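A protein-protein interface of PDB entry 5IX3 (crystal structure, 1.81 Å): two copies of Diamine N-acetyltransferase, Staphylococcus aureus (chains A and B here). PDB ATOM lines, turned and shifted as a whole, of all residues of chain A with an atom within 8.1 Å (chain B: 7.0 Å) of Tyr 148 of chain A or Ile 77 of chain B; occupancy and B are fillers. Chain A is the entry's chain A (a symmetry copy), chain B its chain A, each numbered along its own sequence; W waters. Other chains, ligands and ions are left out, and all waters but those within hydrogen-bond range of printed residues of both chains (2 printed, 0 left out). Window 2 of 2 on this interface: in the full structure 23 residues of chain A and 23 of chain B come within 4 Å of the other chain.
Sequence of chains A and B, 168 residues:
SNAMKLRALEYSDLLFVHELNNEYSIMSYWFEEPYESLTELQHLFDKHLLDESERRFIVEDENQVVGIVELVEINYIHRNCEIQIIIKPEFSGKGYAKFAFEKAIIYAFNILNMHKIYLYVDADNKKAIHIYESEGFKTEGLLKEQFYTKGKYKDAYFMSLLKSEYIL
Water W2 lies within hydrogen-bond range of the backbone carbonyl oxygen (O) of His 78 of chain B (2.8 Å), the side-chain amide nitrogen (ND2) of Asn 80 of chain B (2.8 Å) and the backbone carbonyl oxygen (O) of Glu 145 of chain A (2.8 Å).
Water W1 lies within hydrogen-bond range of O of Gln 146 of chain A and ND2 of Asn 80 of chain B.
Of the 8 printed residues of chain B, 4 touch a printed residue of chain A.
Hydrophobic or aromatic side chains of chain B that line the printed part of chain A: His 78.
Among the printed residues, 8 pairs touch across the chains.
Among the printed residues, no Asp or Glu carboxylate lies within 4 Å of a Lys or Arg side-chain nitrogen of the other chain.
Ile 26 of chain A touches His 78 of chain B.
Tyr 29 of chain A touches Asn 75 of chain B.
Gln 146 of chain A touches His 78 of chain B.
CA of Phe 147 of chain A touches ND1 of His 78 of chain B, at 3.5 Å.
O of Ile 77 of chain B touches CB of Tyr 148 of chain A, at 3.9 Å.
Tyr 153 of chain A touches His 78 of chain B (CE1 to O, 3.4 Å).
OD1 of Asn 75 of chain B is in hydrogen-bond range of N of Ile 77 of chain B.
The side-chain amide oxygen of Asn 75 of chain B sits at hydrogen-bond distance from the backbone NH of His 78 of chain B, 2.8 Å away.
The backbone carbonyl oxygen (O) of Asn 80 of chain B sits at hydrogen-bond distance from the backbone NH (N) of Asn 75 of chain B.
The backbone NH (N) of Asn 80 of chain B is in hydrogen-bond range of the side-chain sulfur (SD) of Met 114 of chain B (3.4 Å).
O of Lys 154 of chain A lies within hydrogen-bond range of N of Gln 146 of chain A, 3.0 Å away.
The backbone carbonyl oxygen of Phe 147 of chain A sits at hydrogen-bond distance from the backbone NH of Lys 154 of chain A (2.7 Å).
Of chain B, only Ile 77 (3.9 Å) and His 78 (2.8 Å) come within 4 Å of Tyr 148 of chain A.
Of chain A, only Tyr 148 (3.9 Å) comes within 4 Å of Ile 77 of chain B.
Of the printed residues of chain B, Ile 26 of chain A touches His 78.
Of the printed residues of chain B, Tyr 29 of chain A touches Asn 75 (3.6 Å).
Of the printed residues of chain B, Phe 147 of chain A touches His 78 (3.5 Å).
The nearest printed residue of chain B that does not touch Tyr 148 of chain A is Arg 79 of chain B (6.0 Å).
A ring nitrogen (ND1) of His 78 of chain B sits at hydrogen-bond distance from the backbone NH (N) of Tyr 148 of chain A (2.8 Å).
The backbone carbonyl oxygen (O) of Gln 146 of chain A lies within hydrogen-bond range of the side-chain amide nitrogen (ND2) of Asn 80 of chain B, at 2.9 Å.
No position is printed for both chains.
Of the 8 pairs that touch across the chains among the printed residues, none has its exchanged pair printed and touching as well.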
ATOM      1  N   SER A  25      -6.441  21.781  -0.929  1.00  0.00           N
ATOM      2  CA  SER A  25      -6.858  22.317  -2.237  1.00  0.00           C
ATOM      3  C   SER A  25      -7.441  23.717  -2.139  1.00  0.00           C
ATOM      4  O   SER A  25      -7.367  24.478  -3.080  1.00  0.00           O
ATOM      5  CB  SER A  25      -7.875  21.394  -2.904  1.00  0.00           C
ATOM      6  OG  SER A  25      -7.211  20.229  -3.342  1.00  0.00           O
ATOM      7  N   ILE A  26      -8.013  24.052  -0.991  1.00  0.00           N
ATOM      8  CA  ILE A  26      -8.498  25.393  -0.755  1.00  0.00           C
ATOM      9  C   ILE A  26      -7.340  26.403  -0.890  1.00  0.00           C
ATOM     10  O   ILE A  26      -6.240  26.196  -0.353  1.00  0.00           O
ATOM     11  CB  ILE A  26      -9.197  25.529   0.633  1.00  0.00           C
ATOM     12  CG1 ILE A  26     -10.149  26.759   0.646  1.00  0.00           C
ATOM     13  CG2 ILE A  26      -8.188  25.516   1.785  1.00  0.00           C
ATOM     14  CD1 ILE A  26     -11.508  26.454   0.029  1.00  0.00           C
ATOM     15  N   MET A  27      -7.622  27.502  -1.573  1.00  0.00           N
ATOM     16  CA  MET A  27      -6.610  28.533  -1.826  1.00  0.00           C
ATOM     17  C   MET A  27      -6.163  29.174  -0.532  1.00  0.00           C
ATOM     18  O   MET A  27      -6.977  29.345   0.418  1.00  0.00           O
ATOM     19  CB  MET A  27      -7.196  29.572  -2.752  1.00  0.00           C
ATOM     20  CG  MET A  27      -7.562  28.962  -4.087  1.00  0.00           C
ATOM     21  SD  MET A  27      -7.448  30.179  -5.381  1.00  0.00           S
ATOM     22  CE  MET A  27      -5.740  30.680  -5.070  1.00  0.00           C
ATOM     23  N   TYR A  29      -4.149  32.213   1.874  1.00  0.00           N
ATOM     24  CA  TYR A  29      -4.038  33.666   1.922  1.00  0.00           C
ATOM     25  C   TYR A  29      -3.012  34.097   2.970  1.00  0.00           C
ATOM     26  O   TYR A  29      -2.917  33.496   4.058  1.00  0.00           O
ATOM     27  CB  TYR A  29      -5.394  34.302   2.220  1.00  0.00           C
ATOM     28  CG  TYR A  29      -6.434  34.037   1.149  1.00  0.00           C
ATOM     29  CD1 TYR A  29      -6.577  34.890   0.050  1.00  0.00           C
ATOM     30  CD2 TYR A  29      -7.255  32.904   1.214  1.00  0.00           C
ATOM     31  CE1 TYR A  29      -7.558  34.635  -0.946  1.00  0.00           C
ATOM     32  CE2 TYR A  29      -8.218  32.644   0.240  1.00  0.00           C
ATOM     33  CZ  TYR A  29      -8.356  33.491  -0.835  1.00  0.00           C
ATOM     34  OH  TYR A  29      -9.320  33.154  -1.758  1.00  0.00           O
ATOM     35  N   PRO A  34      -3.980  36.272  -1.919  1.00  0.00           N
ATOM     36  CA  PRO A  34      -3.815  34.852  -2.188  1.00  0.00           C
ATOM     37  C   PRO A  34      -2.388  34.512  -2.593  1.00  0.00           C
ATOM     38  O   PRO A  34      -1.728  35.301  -3.220  1.00  0.00           O
ATOM     39  CB  PRO A  34      -4.771  34.597  -3.378  1.00  0.00           C
ATOM     40  CG  PRO A  34      -4.832  35.920  -4.096  1.00  0.00           C
ATOM     41  CD  PRO A  34      -4.715  36.963  -3.009  1.00  0.00           C
ATOM     42  N   GLU A 145     -23.393  27.094   1.812  1.00  0.00           N
ATOM     43  CA  GLU A 145     -22.743  27.428   0.492  1.00  0.00           C
ATOM     44  C   GLU A 145     -21.792  28.596   0.608  1.00  0.00           C
ATOM     45  O   GLU A 145     -21.704  29.404  -0.295  1.00  0.00           O
ATOM     46  CB  GLU A 145     -23.816  27.726  -0.557  1.00  0.00           C
ATOM     47  CG  GLU A 145     -24.789  26.573  -0.587  1.00  0.00           C
ATOM     48  CD  GLU A 145     -25.650  26.499  -1.791  1.00  0.00           C
ATOM     49  OE1 GLU A 145     -26.712  25.887  -1.643  1.00  0.00           O
ATOM     50  OE2 GLU A 145     -25.268  27.031  -2.824  1.00  0.00           O
ATOM     51  N   GLN A 146     -21.112  28.693   1.732  1.00  0.00           N
ATOM     52  CA  GLN A 146     -20.249  29.798   2.002  1.00  0.00           C
ATOM     53  C   GLN A 146     -18.852  29.690   1.332  1.00  0.00           C
ATOM     54  O   GLN A 146     -18.162  30.683   1.187  1.00  0.00           O
ATOM     55  CB  GLN A 146     -20.062  29.906   3.514  1.00  0.00           C
ATOM     56  CG  GLN A 146     -19.331  31.168   3.939  1.00  0.00           C
ATOM     57  CD  GLN A 146     -20.158  32.450   3.783  1.00  0.00           C
ATOM     58  OE1 GLN A 146     -21.333  32.439   3.762  1.00  0.00           O
ATOM     59  NE2 GLN A 146     -19.484  33.568   3.652  1.00  0.00           N
ATOM     60  N   PHE A 147     -18.382  28.450   1.045  1.00  0.00           N
ATOM     61  CA  PHE A 147     -17.019  28.187   0.500  1.00  0.00           C
ATOM     62  C   PHE A 147     -17.141  27.255  -0.718  1.00  0.00           C
ATOM     63  O   PHE A 147     -17.943  26.349  -0.756  1.00  0.00           O
ATOM     64  CB  PHE A 147     -16.134  27.578   1.553  1.00  0.00           C
ATOM     65  CG  PHE A 147     -15.842  28.527   2.719  1.00  0.00           C
ATOM     66  CD1 PHE A 147     -14.915  29.568   2.621  1.00  0.00           C
ATOM     67  CD2 PHE A 147     -16.504  28.395   3.929  1.00  0.00           C
ATOM     68  CE1 PHE A 147     -14.630  30.407   3.714  1.00  0.00           C
ATOM     69  CE2 PHE A 147     -16.248  29.272   5.001  1.00  0.00           C
ATOM     70  CZ  PHE A 147     -15.306  30.260   4.899  1.00  0.00           C
ATOM     71  N   TYR A 148     -16.341  27.512  -1.743  1.00  0.00           N
ATOM     72  CA  TYR A 148     -16.367  26.673  -2.905  1.00  0.00           C
ATOM     73  C   TYR A 148     -15.068  25.838  -2.876  1.00  0.00           C
ATOM     74  O   TYR A 148     -13.926  26.394  -2.861  1.00  0.00           O
ATOM     75  CB  TYR A 148     -16.368  27.525  -4.125  1.00  0.00           C
ATOM     76  CG  TYR A 148     -16.399  26.754  -5.398  1.00  0.00           C
ATOM     77  CD1 TYR A 148     -15.252  26.674  -6.233  1.00  0.00           C
ATOM     78  CD2 TYR A 148     -17.557  26.081  -5.781  1.00  0.00           C
ATOM     79  CE1 TYR A 148     -15.326  25.905  -7.418  1.00  0.00           C
ATOM     80  CE2 TYR A 148     -17.627  25.379  -6.962  1.00  0.00           C
ATOM     81  CZ  TYR A 148     -16.503  25.295  -7.759  1.00  0.00           C
ATOM     82  OH  TYR A 148     -16.728  24.594  -8.985  1.00  0.00           O
ATOM     83  N   THR A 149     -15.241  24.561  -2.812  1.00  0.00           N
ATOM     84  CA  THR A 149     -14.076  23.638  -2.569  1.00  0.00           C
ATOM     85  C   THR A 149     -14.292  22.397  -3.364  1.00  0.00           C
ATOM     86  O   THR A 149     -15.369  21.814  -3.371  1.00  0.00           O
ATOM     87  CB  THR A 149     -13.874  23.248  -1.083  1.00  0.00           C
ATOM     88  OG1 THR A 149     -14.586  22.057  -0.808  1.00  0.00           O
ATOM     89  CG2 THR A 149     -14.420  24.318  -0.123  1.00  0.00           C
ATOM     90  N   LYS A 150     -13.296  22.018  -4.162  1.00  0.00           N
ATOM     91  CA  LYS A 150     -13.372  20.798  -4.944  1.00  0.00           C
ATOM     92  C   LYS A 150     -14.624  20.667  -5.754  1.00  0.00           C
ATOM     93  O   LYS A 150     -15.230  19.614  -5.821  1.00  0.00           O
ATOM     94  CB  LYS A 150     -13.172  19.577  -4.041  1.00  0.00           C
ATOM     95  CG  LYS A 150     -11.843  19.540  -3.292  1.00  0.00           C
ATOM     96  CD  LYS A 150     -11.680  18.269  -2.431  1.00  0.00           C
ATOM     97  CE  LYS A 150     -12.946  17.960  -1.609  1.00  0.00           C
ATOM     98  NZ  LYS A 150     -12.797  17.082  -0.408  1.00  0.00           N
ATOM     99  N   GLY A 151     -15.041  21.765  -6.392  1.00  0.00           N
ATOM    100  CA  GLY A 151     -16.157  21.779  -7.310  1.00  0.00           C
ATOM    101  C   GLY A 151     -17.548  21.917  -6.723  1.00  0.00           C
ATOM    102  O   GLY A 151     -18.532  21.891  -7.463  1.00  0.00           O
ATOM    103  N   LYS A 152     -17.632  22.108  -5.410  1.00  0.00           N
ATOM    104  CA  LYS A 152     -18.939  22.205  -4.708  1.00  0.00           C
ATOM    105  C   LYS A 152     -18.924  23.374  -3.738  1.00  0.00           C
ATOM    106  O   LYS A 152     -17.879  23.638  -3.156  1.00  0.00           O
ATOM    107  CB  LYS A 152     -19.188  20.942  -3.906  1.00  0.00           C
ATOM    108  CG  LYS A 152     -19.549  19.738  -4.755  1.00  0.00           C
ATOM    109  CD  LYS A 152     -20.126  18.595  -3.929  1.00  0.00           C
ATOM    110  CE  LYS A 152     -20.268  17.322  -4.754  1.00  0.00           C
ATOM    111  NZ  LYS A 152     -18.956  16.695  -5.095  1.00  0.00           N
ATOM    112  N   TYR A 153     -20.078  24.061  -3.599  1.00  0.00           N
ATOM    113  CA  TYR A 153     -20.261  25.014  -2.516  1.00  0.00           C
ATOM    114  C   TYR A 153     -20.593  24.207  -1.269  1.00  0.00           C
ATOM    115  O   TYR A 153     -21.482  23.319  -1.284  1.00  0.00           O
ATOM    116  CB  TYR A 153     -21.412  26.039  -2.818  1.00  0.00           C
ATOM    117  CG  TYR A 153     -21.081  27.048  -3.889  1.00  0.00           C
ATOM    118  CD1 TYR A 153     -20.241  28.129  -3.619  1.00  0.00           C
ATOM    119  CD2 TYR A 153     -21.465  26.819  -5.239  1.00  0.00           C
ATOM    120  CE1 TYR A 153     -19.882  29.008  -4.612  1.00  0.00           C
ATOM    121  CE2 TYR A 153     -21.115  27.722  -6.233  1.00  0.00           C
ATOM    122  CZ  TYR A 153     -20.344  28.779  -5.927  1.00  0.00           C
ATOM    123  OH  TYR A 153     -20.036  29.686  -6.855  1.00  0.00           O
ATOM    124  N   LYS A 154     -19.914  24.519  -0.192  1.00  0.00           N
ATOM    125  CA  LYS A 154     -20.020  23.770   1.020  1.00  0.00           C
ATOM    126  C   LYS A 154     -20.457  24.694   2.167  1.00  0.00           C
ATOM    127  O   LYS A 154     -20.175  25.847   2.160  1.00  0.00           O
ATOM    128  CB  LYS A 154     -18.649  23.143   1.346  1.00  0.00           C
ATOM    129  CG  LYS A 154     -18.204  22.208   0.215  1.00  0.00           C
ATOM    130  CD  LYS A 154     -17.412  21.001   0.670  1.00  0.00           C
ATOM    131  CE  LYS A 154     -18.255  20.030   1.502  1.00  0.00           C
ATOM    132  NZ  LYS A 154     -17.376  19.129   2.320  1.00  0.00           N
ATOM    133  N   ASP A 155     -21.149  24.102   3.142  1.00  0.00           N
ATOM    134  CA  ASP A 155     -21.602  24.801   4.303  1.00  0.00           C
ATOM    135  C   ASP A 155     -20.504  24.808   5.342  1.00  0.00           C
ATOM    136  O   ASP A 155     -19.673  23.822   5.439  1.00  0.00           O
ATOM    137  CB  ASP A 155     -22.792  24.014   4.863  1.00  0.00           C
ATOM    138  CG  ASP A 155     -23.954  23.923   3.890  1.00  0.00           C
ATOM    139  OD1 ASP A 155     -24.039  24.629   2.860  1.00  0.00           O
ATOM    140  OD2 ASP A 155     -24.868  23.165   4.196  1.00  0.00           O
ATOM    141  N   ILE B  74     -15.237  41.214  -0.858  1.00  0.00           N
ATOM    142  CA  ILE B  74     -15.675  40.568  -2.113  1.00  0.00           C
ATOM    143  C   ILE B  74     -14.666  39.462  -2.385  1.00  0.00           C
ATOM    144  O   ILE B  74     -13.471  39.682  -2.456  1.00  0.00           O
ATOM    145  CB  ILE B  74     -15.790  41.506  -3.309  1.00  0.00           C
ATOM    146  CG1 ILE B  74     -16.767  42.668  -3.010  1.00  0.00           C
ATOM    147  CG2 ILE B  74     -16.223  40.718  -4.530  1.00  0.00           C
ATOM    148  CD1 ILE B  74     -16.827  43.759  -4.023  1.00  0.00           C
ATOM    149  N   ASN B  75     -15.146  38.267  -2.557  1.00  0.00           N
ATOM    150  CA  ASN B  75     -14.278  37.129  -2.807  1.00  0.00           C
ATOM    151  C   ASN B  75     -14.715  36.489  -4.093  1.00  0.00           C
ATOM    152  O   ASN B  75     -15.798  35.951  -4.181  1.00  0.00           O
ATOM    153  CB  ASN B  75     -14.310  36.121  -1.680  1.00  0.00           C
ATOM    154  CG  ASN B  75     -13.289  34.976  -1.892  1.00  0.00           C
ATOM    155  OD1 ASN B  75     -13.387  34.153  -2.798  1.00  0.00           O
ATOM    156  ND2 ASN B  75     -12.368  34.906  -1.007  1.00  0.00           N
ATOM    157  N   TYR B  76     -13.834  36.511  -5.108  1.00  0.00           N
ATOM    158  CA  TYR B  76     -14.195  36.001  -6.453  1.00  0.00           C
ATOM    159  C   TYR B  76     -13.924  34.517  -6.663  1.00  0.00           C
ATOM    160  O   TYR B  76     -14.080  34.035  -7.770  1.00  0.00           O
ATOM    161  CB  TYR B  76     -13.506  36.844  -7.530  1.00  0.00           C
ATOM    162  CG  TYR B  76     -13.889  38.322  -7.564  1.00  0.00           C
ATOM    163  CD1 TYR B  76     -14.985  38.791  -8.256  1.00  0.00           C
ATOM    164  CD2 TYR B  76     -13.216  39.192  -6.775  1.00  0.00           C
ATOM    165  CE1 TYR B  76     -15.337  40.176  -8.200  1.00  0.00           C
ATOM    166  CE2 TYR B  76     -13.540  40.518  -6.688  1.00  0.00           C
ATOM    167  CZ  TYR B  76     -14.576  41.036  -7.412  1.00  0.00           C
ATOM    168  OH  TYR B  76     -14.788  42.420  -7.203  1.00  0.00           O
ATOM    169  N   ILE B  77     -13.529  33.791  -5.627  1.00  0.00           N
ATOM    170  CA  ILE B  77     -13.408  32.357  -5.701  1.00  0.00           C
ATOM    171  C   ILE B  77     -14.677  31.733  -5.090  1.00  0.00           C
ATOM    172  O   ILE B  77     -15.373  30.908  -5.702  1.00  0.00           O
ATOM    173  CB  ILE B  77     -12.143  31.809  -5.034  1.00  0.00           C
ATOM    174  CG1 ILE B  77     -10.855  32.307  -5.679  1.00  0.00           C
ATOM    175  CG2 ILE B  77     -12.222  30.273  -4.928  1.00  0.00           C
ATOM    176  CD1 ILE B  77     -10.743  31.971  -7.114  1.00  0.00           C
ATOM    177  N   HIS B  78     -14.980  32.112  -3.875  1.00  0.00           N
ATOM    178  CA  HIS B  78     -16.149  31.601  -3.207  1.00  0.00           C
ATOM    179  C   HIS B  78     -17.412  32.372  -3.642  1.00  0.00           C
ATOM    180  O   HIS B  78     -18.563  31.903  -3.461  1.00  0.00           O
ATOM    181  CB  HIS B  78     -15.937  31.724  -1.698  1.00  0.00           C
ATOM    182  CG  HIS B  78     -14.733  31.009  -1.227  1.00  0.00           C
ATOM    183  ND1 HIS B  78     -14.541  29.677  -1.482  1.00  0.00           N
ATOM    184  CD2 HIS B  78     -13.608  31.442  -0.623  1.00  0.00           C
ATOM    185  CE1 HIS B  78     -13.365  29.301  -1.030  1.00  0.00           C
ATOM    186  NE2 HIS B  78     -12.773  30.362  -0.510  1.00  0.00           N
ATOM    187  N   ARG B  79     -17.167  33.500  -4.299  1.00  0.00           N
ATOM    188  CA  ARG B  79     -18.277  34.289  -4.882  1.00  0.00           C
ATOM    189  C   ARG B  79     -19.311  34.757  -3.870  1.00  0.00           C
ATOM    190  O   ARG B  79     -20.505  34.447  -3.974  1.00  0.00           O
ATOM    191  CB  ARG B  79     -18.884  33.527  -6.084  1.00  0.00           C
ATOM    192  CG  ARG B  79     -17.764  33.135  -7.099  1.00  0.00           C
ATOM    193  CD  ARG B  79     -18.247  33.139  -8.533  1.00  0.00           C
ATOM    194  NE  ARG B  79     -18.374  34.509  -9.010  1.00  0.00           N
ATOM    195  CZ  ARG B  79     -17.388  35.181  -9.607  1.00  0.00           C
ATOM    196  NH1 ARG B  79     -17.557  36.435  -9.968  1.00  0.00           N
ATOM    197  NH2 ARG B  79     -16.232  34.591  -9.813  1.00  0.00           N
ATOM    198  N   ASN B  80     -18.821  35.440  -2.872  1.00  0.00           N
ATOM    199  CA  ASN B  80     -19.671  36.049  -1.922  1.00  0.00           C
ATOM    200  C   ASN B  80     -19.082  37.316  -1.437  1.00  0.00           C
ATOM    201  O   ASN B  80     -17.863  37.602  -1.610  1.00  0.00           O
ATOM    202  CB  ASN B  80     -20.074  35.086  -0.772  1.00  0.00           C
ATOM    203  CG  ASN B  80     -18.931  34.526  -0.051  1.00  0.00           C
ATOM    204  OD1 ASN B  80     -18.066  35.245   0.410  1.00  0.00           O
ATOM    205  ND2 ASN B  80     -18.918  33.241   0.070  1.00  0.00           N
ATOM    206  N   MET B 114     -21.898  37.104  -8.185  1.00  0.00           N
ATOM    207  CA  MET B 114     -21.757  36.469  -6.867  1.00  0.00           C
ATOM    208  C   MET B 114     -22.766  35.349  -6.704  1.00  0.00           C
ATOM    209  O   MET B 114     -23.798  35.306  -7.381  1.00  0.00           O
ATOM    210  CB  MET B 114     -22.007  37.538  -5.778  1.00  0.00           C
ATOM    211  CG  MET B 114     -20.953  38.621  -5.723  1.00  0.00           C
ATOM    212  SD  MET B 114     -19.374  37.952  -5.040  1.00  0.00           S
ATOM    213  CE  MET B 114     -18.290  38.029  -6.451  1.00  0.00           C
HETATM  214  O   HOH W   1     -16.215  32.530   1.961  1.00  0.00           O
HETATM  215  O   HOH W   2     -20.571  31.663  -1.568  1.00  0.00           O
